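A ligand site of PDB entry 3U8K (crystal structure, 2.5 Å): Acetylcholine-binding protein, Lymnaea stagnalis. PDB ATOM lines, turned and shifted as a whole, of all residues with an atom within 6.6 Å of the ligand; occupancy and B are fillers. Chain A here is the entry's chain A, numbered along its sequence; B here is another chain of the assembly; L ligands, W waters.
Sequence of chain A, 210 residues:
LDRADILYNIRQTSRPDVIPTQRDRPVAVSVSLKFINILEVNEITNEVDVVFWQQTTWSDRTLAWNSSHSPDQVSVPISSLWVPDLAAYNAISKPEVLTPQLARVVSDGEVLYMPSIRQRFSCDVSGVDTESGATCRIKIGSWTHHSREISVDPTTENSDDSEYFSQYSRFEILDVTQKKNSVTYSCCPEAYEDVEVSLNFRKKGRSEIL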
ATOM      1  N   TYR A  89      -3.902  29.437   8.799  1.00  0.00           N
ATOM      2  CA  TYR A  89      -3.992  28.010   8.491  1.00  0.00           C
ATOM      3  C   TYR A  89      -4.017  27.645   7.005  1.00  0.00           C
ATOM      4  O   TYR A  89      -3.515  26.600   6.618  1.00  0.00           O
ATOM      5  CB  TYR A  89      -5.214  27.410   9.163  1.00  0.00           C
ATOM      6  CG  TYR A  89      -5.034  27.190  10.647  1.00  0.00           C
ATOM      7  CD1 TYR A  89      -4.936  28.279  11.524  1.00  0.00           C
ATOM      8  CD2 TYR A  89      -4.974  25.908  11.182  1.00  0.00           C
ATOM      9  CE1 TYR A  89      -4.765  28.082  12.895  1.00  0.00           C
ATOM     10  CE2 TYR A  89      -4.807  25.709  12.545  1.00  0.00           C
ATOM     11  CZ  TYR A  89      -4.697  26.790  13.405  1.00  0.00           C
ATOM     12  OH  TYR A  89      -4.546  26.583  14.765  1.00  0.00           O
ATOM     13  N   GLY A 141      -5.216  31.864  13.804  1.00  0.00           N
ATOM     14  CA  GLY A 141      -5.215  31.625  15.237  1.00  0.00           C
ATOM     15  C   GLY A 141      -3.838  31.308  15.785  1.00  0.00           C
ATOM     16  O   GLY A 141      -2.860  31.245  15.025  1.00  0.00           O
ATOM     17  N   SER A 142      -3.744  31.100  17.096  1.00  0.00           N
ATOM     18  CA  SER A 142      -2.487  30.726  17.727  1.00  0.00           C
ATOM     19  C   SER A 142      -2.065  29.328  17.307  1.00  0.00           C
ATOM     20  O   SER A 142      -2.873  28.382  17.334  1.00  0.00           O
ATOM     21  CB  SER A 142      -2.609  30.774  19.254  1.00  0.00           C
ATOM     22  OG  SER A 142      -1.480  30.164  19.857  1.00  0.00           O
ATOM     23  N   TRP A 143      -0.800  29.171  16.916  1.00  0.00           N
ATOM     24  CA  TRP A 143      -0.357  27.850  16.483  1.00  0.00           C
ATOM     25  C   TRP A 143      -0.242  26.862  17.645  1.00  0.00           C
ATOM     26  O   TRP A 143      -0.587  25.693  17.493  1.00  0.00           O
ATOM     27  CB  TRP A 143       0.979  27.938  15.738  1.00  0.00           C
ATOM     28  CG  TRP A 143       1.235  26.723  14.870  1.00  0.00           C
ATOM     29  CD1 TRP A 143       2.261  25.810  14.999  1.00  0.00           C
ATOM     30  CD2 TRP A 143       0.458  26.294  13.753  1.00  0.00           C
ATOM     31  NE1 TRP A 143       2.177  24.859  14.022  1.00  0.00           N
ATOM     32  CE2 TRP A 143       1.076  25.124  13.237  1.00  0.00           C
ATOM     33  CE3 TRP A 143      -0.690  26.783  13.124  1.00  0.00           C
ATOM     34  CZ2 TRP A 143       0.558  24.421  12.135  1.00  0.00           C
ATOM     35  CZ3 TRP A 143      -1.204  26.099  12.016  1.00  0.00           C
ATOM     36  CH2 TRP A 143      -0.572  24.916  11.541  1.00  0.00           C
ATOM     37  N   THR A 144       0.200  27.315  18.819  1.00  0.00           N
ATOM     38  CA  THR A 144       0.563  26.389  19.898  1.00  0.00           C
ATOM     39  C   THR A 144      -0.106  26.644  21.262  1.00  0.00           C
ATOM     40  O   THR A 144       0.071  25.851  22.187  1.00  0.00           O
ATOM     41  CB  THR A 144       2.098  26.349  20.156  1.00  0.00           C
ATOM     42  OG1 THR A 144       2.521  27.577  20.760  1.00  0.00           O
ATOM     43  CG2 THR A 144       2.892  26.121  18.870  1.00  0.00           C
ATOM     44  N   HIS A 145      -0.830  27.739  21.402  1.00  0.00           N
ATOM     45  CA  HIS A 145      -1.482  28.078  22.663  1.00  0.00           C
ATOM     46  C   HIS A 145      -2.983  27.843  22.584  1.00  0.00           C
ATOM     47  O   HIS A 145      -3.672  28.440  21.743  1.00  0.00           O
ATOM     48  CB  HIS A 145      -1.223  29.541  23.037  1.00  0.00           C
ATOM     49  CG  HIS A 145       0.191  29.832  23.437  1.00  0.00           C
ATOM     50  ND1 HIS A 145       0.682  29.545  24.692  1.00  0.00           N
ATOM     51  CD2 HIS A 145       1.209  30.411  22.761  1.00  0.00           C
ATOM     52  CE1 HIS A 145       1.943  29.925  24.768  1.00  0.00           C
ATOM     53  NE2 HIS A 145       2.283  30.456  23.609  1.00  0.00           N
ATOM     54  N   VAL A 183     -11.925  25.408  18.102  1.00  0.00           N
ATOM     55  CA  VAL A 183     -11.755  24.136  17.414  1.00  0.00           C
ATOM     56  C   VAL A 183     -10.916  23.148  18.222  1.00  0.00           C
ATOM     57  O   VAL A 183      -9.940  23.525  18.858  1.00  0.00           O
ATOM     58  CB  VAL A 183     -11.105  24.351  16.011  1.00  0.00           C
ATOM     59  CG1 VAL A 183     -10.918  23.027  15.301  1.00  0.00           C
ATOM     60  CG2 VAL A 183     -11.927  25.304  15.167  1.00  0.00           C
ATOM     61  N   TYR A 185      -8.685  19.740  17.645  1.00  0.00           N
ATOM     62  CA  TYR A 185      -8.072  18.886  16.632  1.00  0.00           C
ATOM     63  C   TYR A 185      -7.836  17.493  17.208  1.00  0.00           C
ATOM     64  O   TYR A 185      -7.754  17.321  18.416  1.00  0.00           O
ATOM     65  CB  TYR A 185      -6.776  19.516  16.121  1.00  0.00           C
ATOM     66  CG  TYR A 185      -7.008  20.887  15.546  1.00  0.00           C
ATOM     67  CD1 TYR A 185      -6.998  22.008  16.360  1.00  0.00           C
ATOM     68  CD2 TYR A 185      -7.305  21.054  14.200  1.00  0.00           C
ATOM     69  CE1 TYR A 185      -7.242  23.261  15.847  1.00  0.00           C
ATOM     70  CE2 TYR A 185      -7.543  22.312  13.671  1.00  0.00           C
ATOM     71  CZ  TYR A 185      -7.510  23.412  14.500  1.00  0.00           C
ATOM     72  OH  TYR A 185      -7.754  24.665  13.986  1.00  0.00           O
ATOM     73  N   CYS A 187      -5.254  15.684  17.253  1.00  0.00           N
ATOM     74  CA  CYS A 187      -3.954  15.470  17.881  1.00  0.00           C
ATOM     75  C   CYS A 187      -3.980  15.850  19.345  1.00  0.00           C
ATOM     76  O   CYS A 187      -3.225  15.302  20.143  1.00  0.00           O
ATOM     77  CB  CYS A 187      -2.855  16.265  17.170  1.00  0.00           C
ATOM     78  SG  CYS A 187      -3.388  17.339  15.811  1.00  0.00           S
ATOM     79  N   CYS A 188      -4.867  16.787  19.700  1.00  0.00           N
ATOM     80  CA  CYS A 188      -4.817  17.426  21.011  1.00  0.00           C
ATOM     81  C   CYS A 188      -6.163  17.508  21.708  1.00  0.00           C
ATOM     82  O   CYS A 188      -7.195  17.754  21.061  1.00  0.00           O
ATOM     83  CB  CYS A 188      -4.236  18.834  20.873  1.00  0.00           C
ATOM     84  SG  CYS A 188      -2.857  18.947  19.726  1.00  0.00           S
ATOM     85  N   PRO A 189      -6.168  17.334  23.030  1.00  0.00           N
ATOM     86  CA  PRO A 189      -7.403  17.353  23.817  1.00  0.00           C
ATOM     87  C   PRO A 189      -8.009  18.748  24.014  1.00  0.00           C
ATOM     88  O   PRO A 189      -9.214  18.863  24.267  1.00  0.00           O
ATOM     89  CB  PRO A 189      -6.961  16.795  25.167  1.00  0.00           C
ATOM     90  CG  PRO A 189      -5.507  17.140  25.263  1.00  0.00           C
ATOM     91  CD  PRO A 189      -4.974  17.042  23.863  1.00  0.00           C
ATOM     92  N   TYR A 192      -8.696  25.267  20.462  1.00  0.00           N
ATOM     93  CA  TYR A 192      -7.897  26.373  19.944  1.00  0.00           C
ATOM     94  C   TYR A 192      -8.766  27.392  19.226  1.00  0.00           C
ATOM     95  O   TYR A 192      -9.611  27.017  18.396  1.00  0.00           O
ATOM     96  CB  TYR A 192      -6.815  25.844  19.006  1.00  0.00           C
ATOM     97  CG  TYR A 192      -5.813  24.991  19.740  1.00  0.00           C
ATOM     98  CD1 TYR A 192      -6.110  23.675  20.079  1.00  0.00           C
ATOM     99  CD2 TYR A 192      -4.581  25.514  20.149  1.00  0.00           C
ATOM    100  CE1 TYR A 192      -5.210  22.900  20.784  1.00  0.00           C
ATOM    101  CE2 TYR A 192      -3.672  24.736  20.850  1.00  0.00           C
ATOM    102  CZ  TYR A 192      -3.995  23.440  21.164  1.00  0.00           C
ATOM    103  OH  TYR A 192      -3.111  22.657  21.867  1.00  0.00           O
ATOM    104  N   TRP B  53       1.560  19.222   7.970  1.00  0.00           N
ATOM    105  CA  TRP B  53       2.057  19.346   9.332  1.00  0.00           C
ATOM    106  C   TRP B  53       2.997  18.177   9.618  1.00  0.00           C
ATOM    107  O   TRP B  53       2.635  16.998   9.384  1.00  0.00           O
ATOM    108  CB  TRP B  53       0.914  19.287  10.325  1.00  0.00           C
ATOM    109  CG  TRP B  53      -0.066  20.380  10.187  1.00  0.00           C
ATOM    110  CD1 TRP B  53      -0.075  21.391   9.263  1.00  0.00           C
ATOM    111  CD2 TRP B  53      -1.210  20.604  11.017  1.00  0.00           C
ATOM    112  NE1 TRP B  53      -1.147  22.220   9.471  1.00  0.00           N
ATOM    113  CE2 TRP B  53      -1.864  21.754  10.541  1.00  0.00           C
ATOM    114  CE3 TRP B  53      -1.749  19.940  12.121  1.00  0.00           C
ATOM    115  CZ2 TRP B  53      -3.020  22.263  11.133  1.00  0.00           C
ATOM    116  CZ3 TRP B  53      -2.896  20.447  12.708  1.00  0.00           C
ATOM    117  CH2 TRP B  53      -3.529  21.586  12.212  1.00  0.00           C
ATOM    118  N   GLN B  73       2.737  22.640  31.079  1.00  0.00           N
ATOM    119  CA  GLN B  73       3.204  22.809  29.712  1.00  0.00           C
ATOM    120  C   GLN B  73       3.613  24.239  29.409  1.00  0.00           C
ATOM    121  O   GLN B  73       3.009  25.182  29.923  1.00  0.00           O
ATOM    122  CB  GLN B  73       2.145  22.386  28.705  1.00  0.00           C
ATOM    123  CG  GLN B  73       1.659  20.975  28.828  1.00  0.00           C
ATOM    124  CD  GLN B  73       0.800  20.579  27.656  1.00  0.00           C
ATOM    125  OE1 GLN B  73       0.658  21.331  26.686  1.00  0.00           O
ATOM    126  NE2 GLN B  73       0.207  19.398  27.725  1.00  0.00           N
ATOM    127  N   SER B  75       5.276  26.681  25.813  1.00  0.00           N
ATOM    128  CA  SER B  75       5.729  26.755  24.436  1.00  0.00           C
ATOM    129  C   SER B  75       7.113  27.366  24.408  1.00  0.00           C
ATOM    130  O   SER B  75       7.356  28.389  25.049  1.00  0.00           O
ATOM    131  CB  SER B  75       4.771  27.631  23.629  1.00  0.00           C
ATOM    132  OG  SER B  75       3.511  26.994  23.472  1.00  0.00           O
ATOM    133  N   LEU B 102       7.953  27.027  17.289  1.00  0.00           N
ATOM    134  CA  LEU B 102       7.807  26.783  18.708  1.00  0.00           C
ATOM    135  C   LEU B 102       7.488  25.313  18.936  1.00  0.00           C
ATOM    136  O   LEU B 102       6.741  24.733  18.171  1.00  0.00           O
ATOM    137  CB  LEU B 102       6.677  27.639  19.271  1.00  0.00           C
ATOM    138  CG  LEU B 102       6.786  29.163  19.223  1.00  0.00           C
ATOM    139  CD1 LEU B 102       5.451  29.791  19.613  1.00  0.00           C
ATOM    140  CD2 LEU B 102       7.912  29.699  20.117  1.00  0.00           C
ATOM    141  N   ALA B 103       8.067  24.724  19.981  1.00  0.00           N
ATOM    142  CA  ALA B 103       7.697  23.375  20.409  1.00  0.00           C
ATOM    143  C   ALA B 103       6.913  23.437  21.719  1.00  0.00           C
ATOM    144  O   ALA B 103       7.084  24.375  22.493  1.00  0.00           O
ATOM    145  CB  ALA B 103       8.927  22.489  20.563  1.00  0.00           C
ATOM    146  N   ARG B 104       6.063  22.454  21.956  1.00  0.00           N
ATOM    147  CA  ARG B 104       5.321  22.369  23.190  1.00  0.00           C
ATOM    148  C   ARG B 104       6.021  21.361  24.085  1.00  0.00           C
ATOM    149  O   ARG B 104       6.310  20.232  23.653  1.00  0.00           O
ATOM    150  CB  ARG B 104       3.876  21.951  22.919  1.00  0.00           C
ATOM    151  CG  ARG B 104       2.925  22.129  24.101  1.00  0.00           C
ATOM    152  CD  ARG B 104       2.562  23.607  24.363  1.00  0.00           C
ATOM    153  NE  ARG B 104       1.562  23.708  25.424  1.00  0.00           N
ATOM    154  CZ  ARG B 104       1.136  24.833  25.963  1.00  0.00           C
ATOM    155  NH1 ARG B 104       1.604  26.016  25.547  1.00  0.00           N
ATOM    156  NH2 ARG B 104       0.225  24.791  26.923  1.00  0.00           N
ATOM    157  N   LEU B 112       6.610  18.191  21.743  1.00  0.00           N
ATOM    158  CA  LEU B 112       5.868  18.091  20.504  1.00  0.00           C
ATOM    159  C   LEU B 112       6.222  19.285  19.632  1.00  0.00           C
ATOM    160  O   LEU B 112       6.004  20.417  20.016  1.00  0.00           O
ATOM    161  CB  LEU B 112       4.350  18.086  20.769  1.00  0.00           C
ATOM    162  CG  LEU B 112       3.496  18.355  19.513  1.00  0.00           C
ATOM    163  CD1 LEU B 112       3.663  17.257  18.466  1.00  0.00           C
ATOM    164  CD2 LEU B 112       2.021  18.551  19.847  1.00  0.00           C
ATOM    165  N   TYR B 113       6.789  19.011  18.461  1.00  0.00           N
ATOM    166  CA  TYR B 113       7.066  20.054  17.485  1.00  0.00           C
ATOM    167  C   TYR B 113       6.269  19.725  16.223  1.00  0.00           C
ATOM    168  O   TYR B 113       6.368  18.609  15.693  1.00  0.00           O
ATOM    169  CB  TYR B 113       8.576  20.153  17.207  1.00  0.00           C
ATOM    170  CG  TYR B 113       8.953  21.205  16.189  1.00  0.00           C
ATOM    171  CD1 TYR B 113       8.407  22.494  16.247  1.00  0.00           C
ATOM    172  CD2 TYR B 113       9.846  20.923  15.157  1.00  0.00           C
ATOM    173  CE1 TYR B 113       8.746  23.443  15.323  1.00  0.00           C
ATOM    174  CE2 TYR B 113      10.195  21.878  14.227  1.00  0.00           C
ATOM    175  CZ  TYR B 113       9.629  23.137  14.313  1.00  0.00           C
ATOM    176  OH  TYR B 113       9.964  24.108  13.388  1.00  0.00           O
ATOM    177  N   MET B 114       5.443  20.660  15.759  1.00  0.00           N
ATOM    178  CA  MET B 114       4.561  20.386  14.624  1.00  0.00           C
ATOM    179  C   MET B 114       4.382  21.601  13.729  1.00  0.00           C
ATOM    180  O   MET B 114       3.333  22.238  13.730  1.00  0.00           O
ATOM    181  CB  MET B 114       3.208  19.851  15.090  1.00  0.00           C
ATOM    182  CG  MET B 114       2.305  19.339  13.961  1.00  0.00           C
ATOM    183  SD  MET B 114       0.948  18.282  14.532  1.00  0.00           S
ATOM    184  CE  MET B 114      -0.011  19.434  15.548  1.00  0.00           C
ATOM    185  N   PRO B 115       5.414  21.939  12.962  1.00  0.00           N
ATOM    186  CA  PRO B 115       5.316  23.050  12.021  1.00  0.00           C
ATOM    187  C   PRO B 115       4.514  22.658  10.795  1.00  0.00           C
ATOM    188  O   PRO B 115       4.433  21.474  10.451  1.00  0.00           O
ATOM    189  CB  PRO B 115       6.779  23.259  11.611  1.00  0.00           C
ATOM    190  CG  PRO B 115       7.388  21.883  11.706  1.00  0.00           C
ATOM    191  CD  PRO B 115       6.720  21.252  12.905  1.00  0.00           C
HETATM  192  C1  LIG L   1      -2.349  24.083  14.891  1.00  0.00           C
HETATM  193  N1  LIG L   1      -2.876  24.762  16.097  1.00  0.00           N
HETATM  194  C2  LIG L   1      -3.832  24.020  16.952  1.00  0.00           C
HETATM  195  C3  LIG L   1      -3.166  22.869  17.730  1.00  0.00           C
HETATM  196  C4  LIG L   1      -2.359  21.896  16.853  1.00  0.00           C
HETATM  197  N2  LIG L   1      -1.075  22.513  16.476  1.00  0.00           N
HETATM  198  C5  LIG L   1      -1.106  23.207  15.163  1.00  0.00           C
HETATM  199  C6  LIG L   1       2.325  22.392  18.767  1.00  0.00           C
HETATM  200  C7  LIG L   1       1.142  21.957  19.378  1.00  0.00           C
HETATM  201  C8  LIG L   1      -0.041  21.993  18.584  1.00  0.00           C
HETATM  202  C9  LIG L   1       0.023  22.458  17.249  1.00  0.00           C
HETATM  203  C10 LIG L   1       1.290  22.860  16.771  1.00  0.00           C
HETATM  204  N3  LIG L   1       2.413  22.830  17.504  1.00  0.00           N
HETATM  205  O1  LIG L   1       1.201  21.559  20.706  1.00  0.00           O
HETATM  206  C11 LIG L   1      -0.001  21.437  21.467  1.00  0.00           C
HETATM  207  C12 LIG L   1      -0.158  19.986  21.882  1.00  0.00           C
HETATM  208  O   HOH W   1       5.044  23.320  16.415  1.00  0.00           O
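The side-chain hydroxyl of Tyr 89 is in hydrogen-bond range of a nitrogen (N1) of the ligand, 2.8 Å away. A nitrogen (N1) of the ligand sits at hydrogen-bond distance from the backbone carbonyl oxygen (O) of Trp 143 (2.8 Å).
The backbone carbonyl oxygen (O) of Met 114 of chain B lies within hydrogen-bond range of the indole nitrogen (NE1) of Trp 143 (2.9 Å). N of Leu 112 of chain B is in hydrogen-bond range of O of Arg 104 of chain B (2.8 Å). The backbone carbonyl oxygen (O) of Val 183 lies within hydrogen-bond range of the backbone NH (N) of Tyr 192 (2.7 Å). The guanidinium group (NE) of Arg 104 of chain B lies within hydrogen-bond range of the side-chain amide oxygen (OE1) of Gln 73 of chain B. NH1 of Arg 104 of chain B is in hydrogen-bond range of OG of Ser 75 of chain B (3.0 Å). The backbone NH (N) of Thr 144 sits close to the side-chain hydroxyl (OG) of Ser 142, 3.5 Å away. The side-chain hydroxyl (OG1) of Thr 144 lies within hydrogen-bond range of the side-chain hydroxyl (OG) of Ser 75 of chain B, at 2.9 Å. The backbone NH (N) of His 145 sits at hydrogen-bond distance from the side-chain hydroxyl (OG) of Ser 142.
Residues that only touch the ligand: Leu 112 of chain B, Tyr 192, Met 114 of chain B, Arg 104 of chain B, Thr 144, Cys 188, Tyr 185, Ser 142 and Trp 53 of chain B. Hydrophobic or aromatic side chains that line the ligand: Tyr 89, Trp 143, Tyr 185, Tyr 192, Trp 53 of chain B, Leu 112 of chain B and Met 114 of chain B. Within 4 Å of the ligand: Tyr 89, Ser 142, Trp 143, Thr 144, Tyr 185, Cys 188, Tyr 192, Trp 53 of chain B, Arg 104 of chain B, Leu 112 of chain B and Met 114 of chain B. The nearest printed residue that does not touch the ligand is Leu 102 of chain B (4.8 Å).
Water W1 lies within hydrogen-bond range of the backbone NH (N) of Met 114 of chain B (2.8 Å), the backbone carbonyl oxygen (O) of Leu 102 of chain B (2.8 Å) and a nitrogen (N3) of the ligand (2.9 Å).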
